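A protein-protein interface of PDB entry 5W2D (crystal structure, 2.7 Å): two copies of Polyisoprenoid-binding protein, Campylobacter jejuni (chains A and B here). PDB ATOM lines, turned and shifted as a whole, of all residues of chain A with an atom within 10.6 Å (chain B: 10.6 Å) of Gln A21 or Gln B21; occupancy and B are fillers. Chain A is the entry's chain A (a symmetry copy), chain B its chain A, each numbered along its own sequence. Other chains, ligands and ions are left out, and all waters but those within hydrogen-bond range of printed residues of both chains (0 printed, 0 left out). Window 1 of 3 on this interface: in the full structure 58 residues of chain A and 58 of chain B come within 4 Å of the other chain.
Ile A17 touches Asn B24, and with the chains exchanged Asn A24 touches Ile B17.
Ile A17 touches Ser B156, and with the chains exchanged Ser A156 touches Ile B17.
Lys A18 touches Asn B24, and with the chains exchanged Asn A24 touches Lys B18.
His A19 touches Val B25, and with the chains exchanged Val A25 touches His B19.
Positions printed for both chains: 17, 18, 19, 20, 21, 22, 23, 24, 25, 26, 61, 64, 153, 154, 155 and 156.
Gln A21 touches three residues of chain B.
Of chain A, only His A19, Leu A20 and Gln A21 come within 4 Å of Gln B21.
Leu A20 touches four residues of chain B.
Ile A22 touches two residues of chain B.
Ser A23 touches three residues of chain B.
Of chain A, only His A19 and Leu A20 come within 4 Å of Ile B22.
Ser B23 touches just these residues of chain A: Ile A17, Lys A18 and His A19.
Printed residues of chain B within 4 Å of Lys A18: Ser B23 (3.3 Å), Asn B24 (3.2 Å), Leu B155 (3.7 Å) and Ser B156 (2.7 Å).
Of the printed residues of chain B, Asn A24 touches Ile B17 (3.3 Å) and Lys B18 (3.2 Å).
Lys A26 touches none of the printed residues of chain B.
Arg A64 touches none of the printed residues of chain B.
The nearest residue of chain B that does not touch Gln A21 is Ser B23 (4.2 Å).
Among the printed residues, pairs that only touch across the chains: Ile A17 with Ser B23 (3.6 Å), Ile A17 with Asn B24 (3.3 Å), Ile A17 with Leu B155 (3.6 Å), Ile A17 with Ser B156 (3.3 Å), Lys A18 with Ser B23 (3.3 Å), Lys A18 with Asn B24 (3.2 Å), Lys A18 with Leu B155 (3.7 Å), His A19 with Gln B21 (3.8 Å), His A19 with Ile B22 (3.6 Å), His A19 with Val B25 (3.5 Å), His A19 with Thr B154 (3.1 Å), His A19 with Leu B155 (3.7 Å), Leu A20 with Gln B21 (3.7 Å), Leu A20 with Ile B22 (3.8 Å), Leu A20 with Ile B153 (3.6 Å), Gln A21 with His B19 (3.8 Å), Gln A21 with Leu B20 (3.7 Å), Ile A22 with His B19 (3.6 Å), Ile A22 with Leu B20 (3.8 Å), Ser A23 with Ile B17 (3.6 Å), Ser A23 with Lys B18 (3.3 Å), Asn A24 with Ile B17 (3.3 Å), Asn A24 with Lys B18 (3.2 Å), Val A25 with His B19 (3.5 Å), Ile A153 with Leu B20 (3.6 Å), Thr A154 with His B19 (3.1 Å), Leu A155 with Ile B17 (3.6 Å), Leu A155 with Lys B18 (3.7 Å), Leu A155 with His B19 (3.7 Å) and Ser A156 with Ile B17 (3.3 Å).
The backbone carbonyl oxygen (O) of Ile B17 sits at hydrogen-bond distance from the backbone NH (N) of Val A25 (2.5 Å).
The backbone NH (N) of Ser A156 is in hydrogen-bond range of the backbone carbonyl oxygen (O) of Lys B18 (2.7 Å).
N of His B19 lies within hydrogen-bond range of O of Ser A23.
The backbone NH (N) of Leu B20 lies within hydrogen-bond range of the backbone carbonyl oxygen (O) of Thr A154.
N of Gln A21 sits at hydrogen-bond distance from O of Gln B21, at 3.0 Å.
N of His A19 lies within hydrogen-bond range of O of Ser B23 (2.8 Å).
The backbone NH of Val B25 lies within hydrogen-bond range of the backbone carbonyl oxygen of Ile A17 (2.5 Å).
O of Thr B154 is in hydrogen-bond range of N of Leu A20, at 2.8 Å.
The backbone NH of Ser B156 is in hydrogen-bond range of the backbone carbonyl oxygen of Lys A18 (2.7 Å).
Hydrophobic or aromatic side chains of chain B within 4 Å of the printed part of chain A: Ile B17, His B19, Leu B20, Ile B22, Val B25, Ile B153 and Leu B155.
Among the printed residues, no Asp or Glu carboxylate lies within 4 Å of a Lys or Arg side-chain nitrogen of the other chain.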
ATOM      1  N   ILE A  17      -6.376 -19.799  -5.162  1.00  0.00           N
ATOM      2  CA  ILE A  17      -6.704 -21.038  -4.471  1.00  0.00           C
ATOM      3  C   ILE A  17      -8.206 -21.331  -4.500  1.00  0.00           C
ATOM      4  O   ILE A  17      -9.059 -20.437  -4.332  1.00  0.00           O
ATOM      5  CB  ILE A  17      -6.078 -21.114  -3.061  1.00  0.00           C
ATOM      6  CG1 ILE A  17      -6.192 -22.535  -2.504  1.00  0.00           C
ATOM      7  CG2 ILE A  17      -6.623 -20.000  -2.158  1.00  0.00           C
ATOM      8  CD1 ILE A  17      -5.486 -22.746  -1.189  1.00  0.00           C
ATOM      9  N   LYS A  18      -8.506 -22.597  -4.747  1.00  0.00           N
ATOM     10  CA  LYS A  18      -9.868 -23.017  -4.942  1.00  0.00           C
ATOM     11  C   LYS A  18     -10.452 -23.435  -3.599  1.00  0.00           C
ATOM     12  O   LYS A  18      -9.866 -24.291  -2.912  1.00  0.00           O
ATOM     13  CB  LYS A  18      -9.911 -24.177  -5.947  1.00  0.00           C
ATOM     14  CG  LYS A  18      -9.943 -23.748  -7.402  1.00  0.00           C
ATOM     15  CD  LYS A  18      -9.550 -24.902  -8.308  1.00  0.00           C
ATOM     16  CE  LYS A  18      -9.423 -24.436  -9.753  1.00  0.00           C
ATOM     17  NZ  LYS A  18      -9.250 -25.599 -10.666  1.00  0.00           N
ATOM     18  N   HIS A  19     -11.582 -22.826  -3.219  1.00  0.00           N
ATOM     19  CA  HIS A  19     -12.364 -23.345  -2.094  1.00  0.00           C
ATOM     20  C   HIS A  19     -13.851 -23.551  -2.391  1.00  0.00           C
ATOM     21  O   HIS A  19     -14.420 -22.846  -3.237  1.00  0.00           O
ATOM     22  CB  HIS A  19     -12.157 -22.500  -0.817  1.00  0.00           C
ATOM     23  CG  HIS A  19     -12.990 -21.254  -0.743  1.00  0.00           C
ATOM     24  ND1 HIS A  19     -13.219 -20.431  -1.831  1.00  0.00           N
ATOM     25  CD2 HIS A  19     -13.612 -20.666   0.309  1.00  0.00           C
ATOM     26  CE1 HIS A  19     -13.969 -19.408  -1.460  1.00  0.00           C
ATOM     27  NE2 HIS A  19     -14.214 -19.523  -0.164  1.00  0.00           N
ATOM     28  N   LEU A  20     -14.449 -24.514  -1.674  1.00  0.00           N
ATOM     29  CA  LEU A  20     -15.903 -24.746  -1.636  1.00  0.00           C
ATOM     30  C   LEU A  20     -16.663 -23.785  -0.736  1.00  0.00           C
ATOM     31  O   LEU A  20     -16.142 -23.332   0.276  1.00  0.00           O
ATOM     32  CB  LEU A  20     -16.183 -26.165  -1.173  1.00  0.00           C
ATOM     33  CG  LEU A  20     -15.611 -27.233  -2.103  1.00  0.00           C
ATOM     34  CD1 LEU A  20     -15.912 -28.627  -1.572  1.00  0.00           C
ATOM     35  CD2 LEU A  20     -16.134 -27.074  -3.526  1.00  0.00           C
ATOM     36  N   GLN A  21     -17.903 -23.492  -1.116  1.00  0.00           N
ATOM     37  CA  GLN A  21     -18.834 -22.682  -0.328  1.00  0.00           C
ATOM     38  C   GLN A  21     -20.238 -23.277  -0.422  1.00  0.00           C
ATOM     39  O   GLN A  21     -20.835 -23.286  -1.499  1.00  0.00           O
ATOM     40  CB  GLN A  21     -18.881 -21.249  -0.851  1.00  0.00           C
ATOM     41  CG  GLN A  21     -17.686 -20.399  -0.491  1.00  0.00           C
ATOM     42  CD  GLN A  21     -17.949 -18.921  -0.721  1.00  0.00           C
ATOM     43  OE1 GLN A  21     -17.965 -18.449  -1.865  1.00  0.00           O
ATOM     44  NE2 GLN A  21     -18.143 -18.175   0.369  1.00  0.00           N
ATOM     45  N   ILE A  22     -20.761 -23.779   0.697  1.00  0.00           N
ATOM     46  CA  ILE A  22     -22.181 -24.165   0.810  1.00  0.00           C
ATOM     47  C   ILE A  22     -23.082 -22.912   0.720  1.00  0.00           C
ATOM     48  O   ILE A  22     -22.674 -21.822   1.139  1.00  0.00           O
ATOM     49  CB  ILE A  22     -22.437 -24.964   2.116  1.00  0.00           C
ATOM     50  CG1 ILE A  22     -23.460 -26.077   1.888  1.00  0.00           C
ATOM     51  CG2 ILE A  22     -22.849 -24.047   3.267  1.00  0.00           C
ATOM     52  CD1 ILE A  22     -23.423 -27.214   2.899  1.00  0.00           C
ATOM     53  N   SER A  23     -24.264 -23.058   0.112  1.00  0.00           N
ATOM     54  CA  SER A  23     -25.327 -22.024   0.157  1.00  0.00           C
ATOM     55  C   SER A  23     -26.714 -22.632  -0.109  1.00  0.00           C
ATOM     56  O   SER A  23     -26.829 -23.723  -0.698  1.00  0.00           O
ATOM     57  CB  SER A  23     -25.038 -20.787  -0.730  1.00  0.00           C
ATOM     58  OG  SER A  23     -25.576 -20.920  -2.030  1.00  0.00           O
ATOM     59  N   ASN A  24     -27.746 -21.933   0.381  1.00  0.00           N
ATOM     60  CA  ASN A  24     -29.148 -22.326   0.221  1.00  0.00           C
ATOM     61  C   ASN A  24     -29.610 -21.756  -1.086  1.00  0.00           C
ATOM     62  O   ASN A  24     -29.438 -20.559  -1.323  1.00  0.00           O
ATOM     63  CB  ASN A  24     -30.058 -21.723   1.315  1.00  0.00           C
ATOM     64  CG  ASN A  24     -29.641 -22.087   2.734  1.00  0.00           C
ATOM     65  OD1 ASN A  24     -29.508 -21.202   3.594  1.00  0.00           O
ATOM     66  ND2 ASN A  24     -29.459 -23.383   3.000  1.00  0.00           N
ATOM     67  N   VAL A  25     -30.196 -22.598  -1.934  1.00  0.00           N
ATOM     68  CA  VAL A  25     -31.066 -22.078  -2.990  1.00  0.00           C
ATOM     69  C   VAL A  25     -32.477 -22.047  -2.428  1.00  0.00           C
ATOM     70  O   VAL A  25     -32.988 -23.074  -1.927  1.00  0.00           O
ATOM     71  CB  VAL A  25     -31.039 -22.887  -4.294  1.00  0.00           C
ATOM     72  CG1 VAL A  25     -31.639 -22.057  -5.429  1.00  0.00           C
ATOM     73  CG2 VAL A  25     -29.616 -23.275  -4.643  1.00  0.00           C
ATOM     74  N   LYS A  26     -33.071 -20.854  -2.483  1.00  0.00           N
ATOM     75  CA  LYS A  26     -34.414 -20.616  -1.972  1.00  0.00           C
ATOM     76  C   LYS A  26     -35.295 -20.124  -3.124  1.00  0.00           C
ATOM     77  O   LYS A  26     -34.913 -19.218  -3.857  1.00  0.00           O
ATOM     78  CB  LYS A  26     -34.383 -19.626  -0.793  1.00  0.00           C
ATOM     79  N   ASN A  61     -33.446 -15.639 -10.382  1.00  0.00           N
ATOM     80  CA  ASN A  61     -32.335 -15.813 -11.322  1.00  0.00           C
ATOM     81  C   ASN A  61     -33.015 -16.543 -12.451  1.00  0.00           C
ATOM     82  O   ASN A  61     -33.381 -17.736 -12.294  1.00  0.00           O
ATOM     83  CB  ASN A  61     -31.221 -16.708 -10.697  1.00  0.00           C
ATOM     84  CG  ASN A  61     -30.252 -17.270 -11.745  1.00  0.00           C
ATOM     85  OD1 ASN A  61     -30.342 -16.977 -12.934  1.00  0.00           O
ATOM     86  ND2 ASN A  61     -29.328 -18.114 -11.286  1.00  0.00           N
ATOM     87  N   ARG A  64     -31.407 -20.022 -14.136  1.00  0.00           N
ATOM     88  CA  ARG A  64     -31.520 -21.278 -13.334  1.00  0.00           C
ATOM     89  C   ARG A  64     -32.933 -21.874 -13.370  1.00  0.00           C
ATOM     90  O   ARG A  64     -33.088 -23.090 -13.470  1.00  0.00           O
ATOM     91  CB  ARG A  64     -31.086 -21.087 -11.865  1.00  0.00           C
ATOM     92  CG  ARG A  64     -30.602 -22.371 -11.151  1.00  0.00           C
ATOM     93  CD  ARG A  64     -31.027 -22.440  -9.684  1.00  0.00           C
ATOM     94  NE  ARG A  64     -30.313 -21.513  -8.772  1.00  0.00           N
ATOM     95  CZ  ARG A  64     -30.777 -20.318  -8.352  1.00  0.00           C
ATOM     96  NH1 ARG A  64     -31.956 -19.866  -8.751  1.00  0.00           N
ATOM     97  NH2 ARG A  64     -30.063 -19.573  -7.509  1.00  0.00           N
ATOM     98  N   ILE A 153     -23.698 -34.842  -3.260  1.00  0.00           N
ATOM     99  CA  ILE A 153     -22.640 -33.905  -2.901  1.00  0.00           C
ATOM    100  C   ILE A 153     -22.909 -32.480  -3.405  1.00  0.00           C
ATOM    101  O   ILE A 153     -23.045 -31.577  -2.594  1.00  0.00           O
ATOM    102  CB  ILE A 153     -21.249 -34.388  -3.342  1.00  0.00           C
ATOM    103  CG1 ILE A 153     -20.973 -35.797  -2.792  1.00  0.00           C
ATOM    104  CG2 ILE A 153     -20.188 -33.393  -2.875  1.00  0.00           C
ATOM    105  CD1 ILE A 153     -19.714 -36.461  -3.331  1.00  0.00           C
ATOM    106  N   THR A 154     -22.984 -32.276  -4.716  1.00  0.00           N
ATOM    107  CA  THR A 154     -23.122 -30.919  -5.272  1.00  0.00           C
ATOM    108  C   THR A 154     -24.370 -30.223  -4.732  1.00  0.00           C
ATOM    109  O   THR A 154     -24.318 -29.067  -4.314  1.00  0.00           O
ATOM    110  CB  THR A 154     -23.111 -30.934  -6.823  1.00  0.00           C
ATOM    111  OG1 THR A 154     -21.884 -31.533  -7.265  1.00  0.00           O
ATOM    112  CG2 THR A 154     -23.299 -29.481  -7.463  1.00  0.00           C
ATOM    113  N   LEU A 155     -25.472 -30.965  -4.739  1.00  0.00           N
ATOM    114  CA  LEU A 155     -26.778 -30.483  -4.330  1.00  0.00           C
ATOM    115  C   LEU A 155     -27.260 -31.478  -3.314  1.00  0.00           C
ATOM    116  O   LEU A 155     -27.081 -32.696  -3.504  1.00  0.00           O
ATOM    117  CB  LEU A 155     -27.726 -30.460  -5.511  1.00  0.00           C
ATOM    118  CG  LEU A 155     -29.103 -29.839  -5.353  1.00  0.00           C
ATOM    119  CD1 LEU A 155     -29.076 -28.353  -5.634  1.00  0.00           C
ATOM    120  CD2 LEU A 155     -30.052 -30.511  -6.329  1.00  0.00           C
ATOM    121  N   SER A 156     -27.849 -30.931  -2.243  1.00  0.00           N
ATOM    122  CA  SER A 156     -28.280 -31.655  -1.041  1.00  0.00           C
ATOM    123  C   SER A 156     -29.378 -32.647  -1.414  1.00  0.00           C
ATOM    124  O   SER A 156     -30.244 -32.311  -2.239  1.00  0.00           O
ATOM    125  CB  SER A 156     -28.785 -30.622  -0.008  1.00  0.00           C
ATOM    126  OG  SER A 156     -29.677 -31.150   0.965  1.00  0.00           O
ATOM    127  N   ILE B  17     -32.879 -25.444  -0.607  1.00  0.00           N
ATOM    128  CA  ILE B  17     -31.972 -26.558  -0.843  1.00  0.00           C
ATOM    129  C   ILE B  17     -30.508 -26.115  -0.844  1.00  0.00           C
ATOM    130  O   ILE B  17     -30.135 -25.056  -1.388  1.00  0.00           O
ATOM    131  CB  ILE B  17     -32.373 -27.397  -2.077  1.00  0.00           C
ATOM    132  CG1 ILE B  17     -31.587 -28.709  -2.107  1.00  0.00           C
ATOM    133  CG2 ILE B  17     -32.310 -26.554  -3.358  1.00  0.00           C
ATOM    134  CD1 ILE B  17     -32.006 -29.662  -3.197  1.00  0.00           C
ATOM    135  N   LYS B  18     -29.694 -26.934  -0.194  1.00  0.00           N
ATOM    136  CA  LYS B  18     -28.312 -26.599   0.017  1.00  0.00           C
ATOM    137  C   LYS B  18     -27.488 -27.153  -1.139  1.00  0.00           C
ATOM    138  O   LYS B  18     -27.565 -28.361  -1.427  1.00  0.00           O
ATOM    139  CB  LYS B  18     -27.840 -27.181   1.358  1.00  0.00           C
ATOM    140  CG  LYS B  18     -28.129 -26.302   2.561  1.00  0.00           C
ATOM    141  CD  LYS B  18     -28.040 -27.108   3.845  1.00  0.00           C
ATOM    142  CE  LYS B  18     -28.488 -26.274   5.040  1.00  0.00           C
ATOM    143  NZ  LYS B  18     -28.199 -26.987   6.314  1.00  0.00           N
ATOM    144  N   HIS B  19     -26.723 -26.280  -1.804  1.00  0.00           N
ATOM    145  CA  HIS B  19     -25.697 -26.751  -2.739  1.00  0.00           C
ATOM    146  C   HIS B  19     -24.308 -26.150  -2.517  1.00  0.00           C
ATOM    147  O   HIS B  19     -24.191 -25.017  -2.027  1.00  0.00           O
ATOM    148  CB  HIS B  19     -26.150 -26.598  -4.208  1.00  0.00           C
ATOM    149  CG  HIS B  19     -25.961 -25.226  -4.786  1.00  0.00           C
ATOM    150  ND1 HIS B  19     -26.220 -24.066  -4.082  1.00  0.00           N
ATOM    151  CD2 HIS B  19     -25.581 -24.835  -6.028  1.00  0.00           C
ATOM    152  CE1 HIS B  19     -25.980 -23.019  -4.852  1.00  0.00           C
ATOM    153  NE2 HIS B  19     -25.598 -23.459  -6.040  1.00  0.00           N
ATOM    154  N   LEU B  20     -23.282 -26.925  -2.900  1.00  0.00           N
ATOM    155  CA  LEU B  20     -21.881 -26.477  -2.979  1.00  0.00           C
ATOM    156  C   LEU B  20     -21.558 -25.663  -4.222  1.00  0.00           C
ATOM    157  O   LEU B  20     -22.137 -25.879  -5.279  1.00  0.00           O
ATOM    158  CB  LEU B  20     -20.956 -27.680  -2.936  1.00  0.00           C
ATOM    159  CG  LEU B  20     -21.065 -28.488  -1.645  1.00  0.00           C
ATOM    160  CD1 LEU B  20     -20.127 -29.685  -1.675  1.00  0.00           C
ATOM    161  CD2 LEU B  20     -20.795 -27.622  -0.419  1.00  0.00           C
ATOM    162  N   GLN B  21     -20.620 -24.732  -4.077  1.00  0.00           N
ATOM    163  CA  GLN B  21     -20.086 -23.926  -5.178  1.00  0.00           C
ATOM    164  C   GLN B  21     -18.578 -23.753  -5.002  1.00  0.00           C
ATOM    165  O   GLN B  21     -18.137 -23.113  -4.047  1.00  0.00           O
ATOM    166  CB  GLN B  21     -20.732 -22.543  -5.198  1.00  0.00           C
ATOM    167  CG  GLN B  21     -22.145 -22.507  -5.729  1.00  0.00           C
ATOM    168  CD  GLN B  21     -22.594 -21.093  -6.056  1.00  0.00           C
ATOM    169  OE1 GLN B  21     -22.891 -20.297  -5.158  1.00  0.00           O
ATOM    170  NE2 GLN B  21     -22.661 -20.777  -7.351  1.00  0.00           N
ATOM    171  N   ILE B  22     -17.791 -24.323  -5.914  1.00  0.00           N
ATOM    172  CA  ILE B  22     -16.345 -24.044  -6.006  1.00  0.00           C
ATOM    173  C   ILE B  22     -16.113 -22.578  -6.440  1.00  0.00           C
ATOM    174  O   ILE B  22     -16.928 -22.012  -7.179  1.00  0.00           O
ATOM    175  CB  ILE B  22     -15.646 -25.044  -6.965  1.00  0.00           C
ATOM    176  CG1 ILE B  22     -14.256 -25.420  -6.449  1.00  0.00           C
ATOM    177  CG2 ILE B  22     -15.591 -24.511  -8.396  1.00  0.00           C
ATOM    178  CD1 ILE B  22     -13.692 -26.727  -6.989  1.00  0.00           C
ATOM    179  N   SER B  23     -15.049 -21.954  -5.925  1.00  0.00           N
ATOM    180  CA  SER B  23     -14.562 -20.644  -6.423  1.00  0.00           C
ATOM    181  C   SER B  23     -13.079 -20.428  -6.080  1.00  0.00           C
ATOM    182  O   SER B  23     -12.538 -21.066  -5.159  1.00  0.00           O
ATOM    183  CB  SER B  23     -15.451 -19.445  -6.006  1.00  0.00           C
ATOM    184  OG  SER B  23     -15.026 -18.856  -4.793  1.00  0.00           O
ATOM    185  N   ASN B  24     -12.432 -19.564  -6.872  1.00  0.00           N
ATOM    186  CA  ASN B  24     -11.023 -19.202  -6.706  1.00  0.00           C
ATOM    187  C   ASN B  24     -10.979 -18.066  -5.729  1.00  0.00           C
ATOM    188  O   ASN B  24     -11.690 -17.077  -5.914  1.00  0.00           O
ATOM    189  CB  ASN B  24     -10.389 -18.681  -8.017  1.00  0.00           C
ATOM    190  CG  ASN B  24     -10.473 -19.667  -9.176  1.00  0.00           C
ATOM    191  OD1 ASN B  24     -10.914 -19.302 -10.277  1.00  0.00           O
ATOM    192  ND2 ASN B  24     -10.031 -20.907  -8.952  1.00  0.00           N
ATOM    193  N   VAL B  25     -10.154 -18.197  -4.693  1.00  0.00           N
ATOM    194  CA  VAL B  25      -9.705 -17.009  -3.966  1.00  0.00           C
ATOM    195  C   VAL B  25      -8.415 -16.547  -4.624  1.00  0.00           C
ATOM    196  O   VAL B  25      -7.457 -17.338  -4.774  1.00  0.00           O
ATOM    197  CB  VAL B  25      -9.480 -17.227  -2.464  1.00  0.00           C
ATOM    198  CG1 VAL B  25      -9.415 -15.877  -1.750  1.00  0.00           C
ATOM    199  CG2 VAL B  25     -10.602 -18.062  -1.879  1.00  0.00           C
ATOM    200  N   LYS B  26      -8.426 -15.281  -5.042  1.00  0.00           N
ATOM    201  CA  LYS B  26      -7.294 -14.664  -5.718  1.00  0.00           C
ATOM    202  C   LYS B  26      -6.831 -13.459  -4.894  1.00  0.00           C
ATOM    203  O   LYS B  26      -7.640 -12.628  -4.496  1.00  0.00           O
ATOM    204  CB  LYS B  26      -7.664 -14.279  -7.163  1.00  0.00           C
ATOM    205  N   ASN B  61     -11.115  -8.051   0.456  1.00  0.00           N
ATOM    206  CA  ASN B  61     -12.107  -8.362   1.489  1.00  0.00           C
ATOM    207  C   ASN B  61     -11.272  -8.261   2.739  1.00  0.00           C
ATOM    208  O   ASN B  61     -10.398  -9.132   2.980  1.00  0.00           O
ATOM    209  CB  ASN B  61     -12.642  -9.817   1.317  1.00  0.00           C
ATOM    210  CG  ASN B  61     -13.343 -10.344   2.575  1.00  0.00           C
ATOM    211  OD1 ASN B  61     -13.497  -9.646   3.574  1.00  0.00           O
ATOM    212  ND2 ASN B  61     -13.746 -11.614   2.524  1.00  0.00           N
ATOM    213  N   ARG B  64     -11.289 -11.248   5.672  1.00  0.00           N
ATOM    214  CA  ARG B  64     -10.555 -12.512   5.355  1.00  0.00           C
ATOM    215  C   ARG B  64      -9.034 -12.356   5.477  1.00  0.00           C
ATOM    216  O   ARG B  64      -8.359 -13.250   5.984  1.00  0.00           O
ATOM    217  CB  ARG B  64     -10.899 -13.066   3.957  1.00  0.00           C
ATOM    218  CG  ARG B  64     -10.692 -14.589   3.785  1.00  0.00           C
ATOM    219  CD  ARG B  64     -10.157 -14.970   2.405  1.00  0.00           C
ATOM    220  NE  ARG B  64     -11.128 -14.849   1.290  1.00  0.00           N
ATOM    221  CZ  ARG B  64     -11.216 -13.807   0.439  1.00  0.00           C
ATOM    222  NH1 ARG B  64     -10.403 -12.767   0.550  1.00  0.00           N
ATOM    223  NH2 ARG B  64     -12.111 -13.811  -0.548  1.00  0.00           N
ATOM    224  N   ILE B 153     -10.560 -30.707   1.409  1.00  0.00           N
ATOM    225  CA  ILE B 153     -11.890 -30.538   0.837  1.00  0.00           C
ATOM    226  C   ILE B 153     -12.333 -29.070   0.783  1.00  0.00           C
ATOM    227  O   ILE B 153     -12.547 -28.551  -0.303  1.00  0.00           O
ATOM    228  CB  ILE B 153     -12.949 -31.403   1.538  1.00  0.00           C
ATOM    229  CG1 ILE B 153     -12.515 -32.879   1.544  1.00  0.00           C
ATOM    230  CG2 ILE B 153     -14.298 -31.226   0.845  1.00  0.00           C
ATOM    231  CD1 ILE B 153     -13.384 -33.800   2.389  1.00  0.00           C
ATOM    232  N   THR B 154     -12.472 -28.407   1.927  1.00  0.00           N
ATOM    233  CA  THR B 154     -13.005 -27.035   1.956  1.00  0.00           C
ATOM    234  C   THR B 154     -12.160 -26.092   1.099  1.00  0.00           C
ATOM    235  O   THR B 154     -12.688 -25.312   0.308  1.00  0.00           O
ATOM    236  CB  THR B 154     -13.142 -26.507   3.407  1.00  0.00           C
ATOM    237  OG1 THR B 154     -14.004 -27.394   4.136  1.00  0.00           O
ATOM    238  CG2 THR B 154     -13.682 -25.004   3.478  1.00  0.00           C
ATOM    239  N   LEU B 155     -10.847 -26.206   1.272  1.00  0.00           N
ATOM    240  CA  LEU B 155      -9.867 -25.368   0.608  1.00  0.00           C
ATOM    241  C   LEU B 155      -8.904 -26.326  -0.031  1.00  0.00           C
ATOM    242  O   LEU B 155      -8.533 -27.340   0.590  1.00  0.00           O
ATOM    243  CB  LEU B 155      -9.136 -24.509   1.619  1.00  0.00           C
ATOM    244  CG  LEU B 155      -8.176 -23.436   1.134  1.00  0.00           C
ATOM    245  CD1 LEU B 155      -8.890 -22.128   0.876  1.00  0.00           C
ATOM    246  CD2 LEU B 155      -7.114 -23.220   2.199  1.00  0.00           C
ATOM    247  N   SER B 156      -8.532 -25.989  -1.273  1.00  0.00           N
ATOM    248  CA  SER B 156      -7.720 -26.814  -2.176  1.00  0.00           C
ATOM    249  C   SER B 156      -6.331 -27.005  -1.574  1.00  0.00           C
ATOM    250  O   SER B 156      -5.783 -26.051  -0.999  1.00  0.00           O
ATOM    251  CB  SER B 156      -7.646 -26.101  -3.545  1.00  0.00           C
ATOM    252  OG  SER B 156      -6.530 -26.477  -4.344  1.00  0.00           O
